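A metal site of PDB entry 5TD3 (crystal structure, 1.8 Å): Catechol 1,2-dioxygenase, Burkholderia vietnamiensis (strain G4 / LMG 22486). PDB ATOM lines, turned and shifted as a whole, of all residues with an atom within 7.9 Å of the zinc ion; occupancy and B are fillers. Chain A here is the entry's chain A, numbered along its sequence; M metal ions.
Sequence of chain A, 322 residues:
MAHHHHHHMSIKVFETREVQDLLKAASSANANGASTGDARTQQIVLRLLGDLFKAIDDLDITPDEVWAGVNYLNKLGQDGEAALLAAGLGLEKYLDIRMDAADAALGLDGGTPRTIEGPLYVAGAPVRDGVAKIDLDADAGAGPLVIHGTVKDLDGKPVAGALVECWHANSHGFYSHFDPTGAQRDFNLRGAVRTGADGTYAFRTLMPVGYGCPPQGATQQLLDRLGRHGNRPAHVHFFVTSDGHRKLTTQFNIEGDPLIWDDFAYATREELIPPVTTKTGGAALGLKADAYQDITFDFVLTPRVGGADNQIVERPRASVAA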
ATOM      1  N   ILE A 116      11.709   6.100  -5.948  1.00  0.00           N
ATOM      2  CA  ILE A 116      13.022   6.657  -5.604  1.00  0.00           C
ATOM      3  C   ILE A 116      12.930   8.173  -5.426  1.00  0.00           C
ATOM      4  O   ILE A 116      12.134   8.868  -6.061  1.00  0.00           O
ATOM      5  CB  ILE A 116      14.101   6.305  -6.645  1.00  0.00           C
ATOM      6  CG1 ILE A 116      13.897   7.093  -7.945  1.00  0.00           C
ATOM      7  CG2 ILE A 116      14.150   4.784  -6.887  1.00  0.00           C
ATOM      8  CD1 ILE A 116      14.923   6.784  -9.009  1.00  0.00           C
ATOM      9  N   GLU A 117      13.773   8.675  -4.530  1.00  0.00           N
ATOM     10  CA  GLU A 117      13.852  10.103  -4.286  1.00  0.00           C
ATOM     11  C   GLU A 117      14.521  10.824  -5.456  1.00  0.00           C
ATOM     12  O   GLU A 117      14.112  11.922  -5.826  1.00  0.00           O
ATOM     13  CB  GLU A 117      14.627  10.367  -2.986  1.00  0.00           C
ATOM     14  CG  GLU A 117      14.717  11.845  -2.599  1.00  0.00           C
ATOM     15  CD  GLU A 117      15.503  12.057  -1.327  1.00  0.00           C
ATOM     16  OE1 GLU A 117      15.454  11.167  -0.457  1.00  0.00           O
ATOM     17  OE2 GLU A 117      16.148  13.127  -1.194  1.00  0.00           O
ATOM     18  N   GLY A 118      15.540  10.194  -6.052  1.00  0.00           N
ATOM     19  CA  GLY A 118      16.427  10.867  -6.974  1.00  0.00           C
ATOM     20  C   GLY A 118      17.339  11.840  -6.234  1.00  0.00           C
ATOM     21  O   GLY A 118      17.192  12.063  -5.030  1.00  0.00           O
ATOM     22  N   PRO A 119      18.287  12.450  -6.948  1.00  0.00           N
ATOM     23  CA  PRO A 119      19.321  13.248  -6.264  1.00  0.00           C
ATOM     24  C   PRO A 119      19.083  14.744  -6.267  1.00  0.00           C
ATOM     25  O   PRO A 119      20.020  15.513  -6.001  1.00  0.00           O
ATOM     26  CB  PRO A 119      20.582  12.902  -7.071  1.00  0.00           C
ATOM     27  CG  PRO A 119      20.050  12.784  -8.469  1.00  0.00           C
ATOM     28  CD  PRO A 119      18.665  12.137  -8.329  1.00  0.00           C
ATOM     29  N   LEU A 120      17.865  15.196  -6.565  1.00  0.00           N
ATOM     30  CA  LEU A 120      17.617  16.610  -6.850  1.00  0.00           C
ATOM     31  C   LEU A 120      16.671  17.280  -5.868  1.00  0.00           C
ATOM     32  O   LEU A 120      16.108  18.339  -6.184  1.00  0.00           O
ATOM     33  CB  LEU A 120      17.075  16.756  -8.279  1.00  0.00           C
ATOM     34  CG  LEU A 120      18.029  16.174  -9.342  1.00  0.00           C
ATOM     35  CD1 LEU A 120      17.482  16.404 -10.735  1.00  0.00           C
ATOM     36  CD2 LEU A 120      19.392  16.787  -9.190  1.00  0.00           C
ATOM     37  N   TYR A 121      16.457  16.715  -4.679  1.00  0.00           N
ATOM     38  CA  TYR A 121      15.713  17.458  -3.665  1.00  0.00           C
ATOM     39  C   TYR A 121      16.485  18.689  -3.192  1.00  0.00           C
ATOM     40  O   TYR A 121      17.723  18.705  -3.159  1.00  0.00           O
ATOM     41  CB  TYR A 121      15.400  16.552  -2.475  1.00  0.00           C
ATOM     42  CG  TYR A 121      14.660  17.254  -1.348  1.00  0.00           C
ATOM     43  CD1 TYR A 121      13.323  17.589  -1.458  1.00  0.00           C
ATOM     44  CD2 TYR A 121      15.320  17.576  -0.167  1.00  0.00           C
ATOM     45  CE1 TYR A 121      12.645  18.202  -0.414  1.00  0.00           C
ATOM     46  CE2 TYR A 121      14.659  18.190   0.877  1.00  0.00           C
ATOM     47  CZ  TYR A 121      13.328  18.498   0.752  1.00  0.00           C
ATOM     48  OH  TYR A 121      12.691  19.116   1.811  1.00  0.00           O
ATOM     49  N   TRP A 167       8.500  18.632  -6.067  1.00  0.00           N
ATOM     50  CA  TRP A 167       9.499  19.274  -6.928  1.00  0.00           C
ATOM     51  C   TRP A 167       9.520  18.560  -8.269  1.00  0.00           C
ATOM     52  O   TRP A 167       9.277  17.352  -8.350  1.00  0.00           O
ATOM     53  CB  TRP A 167      10.898  19.307  -6.293  1.00  0.00           C
ATOM     54  CG  TRP A 167      11.606  17.965  -6.024  1.00  0.00           C
ATOM     55  CD1 TRP A 167      12.667  17.437  -6.706  1.00  0.00           C
ATOM     56  CD2 TRP A 167      11.335  17.042  -4.949  1.00  0.00           C
ATOM     57  NE1 TRP A 167      13.049  16.241  -6.140  1.00  0.00           N
ATOM     58  CE2 TRP A 167      12.250  15.984  -5.063  1.00  0.00           C
ATOM     59  CE3 TRP A 167      10.387  17.023  -3.901  1.00  0.00           C
ATOM     60  CZ2 TRP A 167      12.251  14.893  -4.178  1.00  0.00           C
ATOM     61  CZ3 TRP A 167      10.393  15.944  -3.029  1.00  0.00           C
ATOM     62  CH2 TRP A 167      11.313  14.901  -3.169  1.00  0.00           C
ATOM     63  N   HIS A 168       9.782  19.324  -9.331  1.00  0.00           N
ATOM     64  CA  HIS A 168       9.812  18.752 -10.667  1.00  0.00           C
ATOM     65  C   HIS A 168      10.540  19.705 -11.601  1.00  0.00           C
ATOM     66  O   HIS A 168      10.899  20.830 -11.232  1.00  0.00           O
ATOM     67  CB  HIS A 168       8.392  18.445 -11.179  1.00  0.00           C
ATOM     68  CG  HIS A 168       7.560  19.658 -11.424  1.00  0.00           C
ATOM     69  ND1 HIS A 168       7.663  20.417 -12.568  1.00  0.00           N
ATOM     70  CD2 HIS A 168       6.635  20.268 -10.646  1.00  0.00           C
ATOM     71  CE1 HIS A 168       6.816  21.436 -12.496  1.00  0.00           C
ATOM     72  NE2 HIS A 168       6.185  21.366 -11.343  1.00  0.00           N
ATOM     73  N   ALA A 169      10.752  19.227 -12.826  1.00  0.00           N
ATOM     74  CA  ALA A 169      11.561  19.925 -13.833  1.00  0.00           C
ATOM     75  C   ALA A 169      10.726  20.902 -14.660  1.00  0.00           C
ATOM     76  O   ALA A 169       9.489  20.856 -14.671  1.00  0.00           O
ATOM     77  CB  ALA A 169      12.243  18.904 -14.737  1.00  0.00           C
ATOM     78  N   GLY A 173      13.644  20.105 -18.967  1.00  0.00           N
ATOM     79  CA  GLY A 173      14.081  18.994 -18.164  1.00  0.00           C
ATOM     80  C   GLY A 173      15.048  19.377 -17.076  1.00  0.00           C
ATOM     81  O   GLY A 173      15.693  18.491 -16.503  1.00  0.00           O
ATOM     82  N   TYR A 175      15.933  21.235 -13.322  1.00  0.00           N
ATOM     83  CA  TYR A 175      15.401  21.602 -12.023  1.00  0.00           C
ATOM     84  C   TYR A 175      16.082  22.851 -11.505  1.00  0.00           C
ATOM     85  O   TYR A 175      17.280  23.040 -11.683  1.00  0.00           O
ATOM     86  CB  TYR A 175      15.633  20.501 -10.990  1.00  0.00           C
ATOM     87  CG  TYR A 175      14.849  19.242 -11.178  1.00  0.00           C
ATOM     88  CD1 TYR A 175      15.113  18.366 -12.234  1.00  0.00           C
ATOM     89  CD2 TYR A 175      13.871  18.874 -10.266  1.00  0.00           C
ATOM     90  CE1 TYR A 175      14.399  17.200 -12.387  1.00  0.00           C
ATOM     91  CE2 TYR A 175      13.163  17.712 -10.404  1.00  0.00           C
ATOM     92  CZ  TYR A 175      13.427  16.873 -11.458  1.00  0.00           C
ATOM     93  OH  TYR A 175      12.692  15.709 -11.552  1.00  0.00           O
ATOM     94  N   VAL A 209       8.791  18.188 -18.186  1.00  0.00           N
ATOM     95  CA  VAL A 209       9.302  17.367 -19.275  1.00  0.00           C
ATOM     96  C   VAL A 209      10.358  16.443 -18.685  1.00  0.00           C
ATOM     97  O   VAL A 209      10.966  16.762 -17.663  1.00  0.00           O
ATOM     98  CB  VAL A 209       9.878  18.279 -20.387  1.00  0.00           C
ATOM     99  CG1 VAL A 209      10.644  17.504 -21.439  1.00  0.00           C
ATOM    100  CG2 VAL A 209       8.741  19.056 -21.017  1.00  0.00           C
ATOM    101  N   GLY A 210      10.561  15.283 -19.319  1.00  0.00           N
ATOM    102  CA  GLY A 210      11.483  14.308 -18.794  1.00  0.00           C
ATOM    103  C   GLY A 210      12.919  14.808 -18.709  1.00  0.00           C
ATOM    104  O   GLY A 210      13.359  15.669 -19.479  1.00  0.00           O
ATOM    105  N   TYR A 211      13.655  14.218 -17.784  1.00  0.00           N
ATOM    106  CA  TYR A 211      15.033  14.544 -17.455  1.00  0.00           C
ATOM    107  C   TYR A 211      16.002  13.654 -18.237  1.00  0.00           C
ATOM    108  O   TYR A 211      15.697  12.502 -18.550  1.00  0.00           O
ATOM    109  CB  TYR A 211      15.215  14.360 -15.927  1.00  0.00           C
ATOM    110  CG  TYR A 211      16.634  14.320 -15.420  1.00  0.00           C
ATOM    111  CD1 TYR A 211      17.390  13.143 -15.498  1.00  0.00           C
ATOM    112  CD2 TYR A 211      17.210  15.414 -14.819  1.00  0.00           C
ATOM    113  CE1 TYR A 211      18.697  13.093 -15.040  1.00  0.00           C
ATOM    114  CE2 TYR A 211      18.517  15.371 -14.337  1.00  0.00           C
ATOM    115  CZ  TYR A 211      19.255  14.204 -14.456  1.00  0.00           C
ATOM    116  OH  TYR A 211      20.550  14.172 -13.986  1.00  0.00           O
ATOM    117  N   ARG A 232      14.724   9.959 -18.352  1.00  0.00           N
ATOM    118  CA  ARG A 232      13.557   9.671 -17.529  1.00  0.00           C
ATOM    119  C   ARG A 232      12.300  10.206 -18.198  1.00  0.00           C
ATOM    120  O   ARG A 232      12.349  11.247 -18.849  1.00  0.00           O
ATOM    121  CB  ARG A 232      13.672  10.328 -16.142  1.00  0.00           C
ATOM    122  CG  ARG A 232      14.968  10.016 -15.419  1.00  0.00           C
ATOM    123  CD  ARG A 232      14.805  10.138 -13.926  1.00  0.00           C
ATOM    124  NE  ARG A 232      13.895   9.132 -13.413  1.00  0.00           N
ATOM    125  CZ  ARG A 232      13.250   9.237 -12.268  1.00  0.00           C
ATOM    126  NH1 ARG A 232      13.411  10.319 -11.500  1.00  0.00           N
ATOM    127  NH2 ARG A 232      12.444   8.270 -11.880  1.00  0.00           N
ATOM    128  N   PRO A 233      11.159   9.538 -18.023  1.00  0.00           N
ATOM    129  CA  PRO A 233       9.882  10.122 -18.447  1.00  0.00           C
ATOM    130  C   PRO A 233       9.566  11.322 -17.565  1.00  0.00           C
ATOM    131  O   PRO A 233      10.120  11.490 -16.476  1.00  0.00           O
ATOM    132  CB  PRO A 233       8.881   8.982 -18.232  1.00  0.00           C
ATOM    133  CG  PRO A 233       9.489   8.198 -17.080  1.00  0.00           C
ATOM    134  CD  PRO A 233      10.969   8.232 -17.358  1.00  0.00           C
ATOM    135  N   ALA A 234       8.648  12.171 -18.041  1.00  0.00           N
ATOM    136  CA  ALA A 234       8.198  13.292 -17.217  1.00  0.00           C
ATOM    137  C   ALA A 234       7.560  12.765 -15.942  1.00  0.00           C
ATOM    138  O   ALA A 234       6.803  11.787 -15.953  1.00  0.00           O
ATOM    139  CB  ALA A 234       7.217  14.174 -17.980  1.00  0.00           C
ATOM    140  N   HIS A 235       7.844  13.435 -14.829  1.00  0.00           N
ATOM    141  CA  HIS A 235       7.385  12.958 -13.520  1.00  0.00           C
ATOM    142  C   HIS A 235       7.391  14.119 -12.545  1.00  0.00           C
ATOM    143  O   HIS A 235       7.935  15.187 -12.816  1.00  0.00           O
ATOM    144  CB  HIS A 235       8.279  11.831 -13.009  1.00  0.00           C
ATOM    145  CG  HIS A 235       9.712  12.248 -12.879  1.00  0.00           C
ATOM    146  ND1 HIS A 235      10.560  12.321 -13.960  1.00  0.00           N
ATOM    147  CD2 HIS A 235      10.425  12.667 -11.801  1.00  0.00           C
ATOM    148  CE1 HIS A 235      11.749  12.754 -13.553  1.00  0.00           C
ATOM    149  NE2 HIS A 235      11.686  12.970 -12.252  1.00  0.00           N
ATOM    150  N   VAL A 236       6.791  13.890 -11.388  1.00  0.00           N
ATOM    151  CA  VAL A 236       6.723  14.858 -10.311  1.00  0.00           C
ATOM    152  C   VAL A 236       7.081  14.126  -9.033  1.00  0.00           C
ATOM    153  O   VAL A 236       6.572  13.028  -8.793  1.00  0.00           O
ATOM    154  CB  VAL A 236       5.323  15.485 -10.173  1.00  0.00           C
ATOM    155  CG1 VAL A 236       5.292  16.456  -9.009  1.00  0.00           C
ATOM    156  CG2 VAL A 236       4.924  16.211 -11.465  1.00  0.00           C
ATOM    157  N   HIS A 237       7.972  14.713  -8.227  1.00  0.00           N
ATOM    158  CA  HIS A 237       8.392  14.127  -6.960  1.00  0.00           C
ATOM    159  C   HIS A 237       7.534  14.620  -5.806  1.00  0.00           C
ATOM    160  O   HIS A 237       7.099  15.782  -5.803  1.00  0.00           O
ATOM    161  CB  HIS A 237       9.846  14.479  -6.599  1.00  0.00           C
ATOM    162  CG  HIS A 237      10.871  14.003  -7.581  1.00  0.00           C
ATOM    163  ND1 HIS A 237      11.520  12.796  -7.451  1.00  0.00           N
ATOM    164  CD2 HIS A 237      11.394  14.601  -8.680  1.00  0.00           C
ATOM    165  CE1 HIS A 237      12.380  12.653  -8.439  1.00  0.00           C
ATOM    166  NE2 HIS A 237      12.332  13.726  -9.202  1.00  0.00           N
ATOM    167  N   GLN A 251       6.562   9.451  -6.249  1.00  0.00           N
ATOM    168  CA  GLN A 251       6.449  10.275  -7.435  1.00  0.00           C
ATOM    169  C   GLN A 251       5.194   9.837  -8.182  1.00  0.00           C
ATOM    170  O   GLN A 251       4.555   8.847  -7.837  1.00  0.00           O
ATOM    171  CB  GLN A 251       7.664  10.134  -8.343  1.00  0.00           C
ATOM    172  CG  GLN A 251       7.540   9.003  -9.357  1.00  0.00           C
ATOM    173  CD  GLN A 251       8.742   8.901 -10.284  1.00  0.00           C
ATOM    174  OE1 GLN A 251       8.661   8.314 -11.357  1.00  0.00           O
ATOM    175  NE2 GLN A 251       9.855   9.471  -9.856  1.00  0.00           N
HETATM  176 ZN    ZN M   1      13.016  13.973 -11.013  1.00  0.00          ZN
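Merely in contact with the zinc ion: Arg 232 (3.7 Å). Within 4 Å of the zinc ion: Tyr 175, Arg 232, His 235 and His 237.
NE2 of Gln 251 lies close to NH2 of Arg 232 (3.5 Å). N of His 237 lies within hydrogen-bond range of O of Trp 167 (2.9 Å). The backbone carbonyl oxygen (O) of Glu 117 sits at hydrogen-bond distance from a ring nitrogen (ND1) of His 237, 3.2 Å away. A ring nitrogen (NE2) of His 235 sits close to the guanidinium group (NH1) of Arg 232, at 3.3 Å. The backbone carbonyl oxygen (O) of Tyr 211 sits at hydrogen-bond distance from the backbone NH (N) of Arg 232, at 2.7 Å. ND1 of His 235 is in hydrogen-bond range of O of Pro 233, at 2.7 Å.
The zinc ion is bound by the side-chain hydroxyl (OH) of Tyr 175 (1.8 Å), a ring nitrogen (NE2) of His 237 (2.0 Å) and a ring nitrogen (NE2) of His 235 (2.1 Å). The zinc ion has three donor atoms within binding distance.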
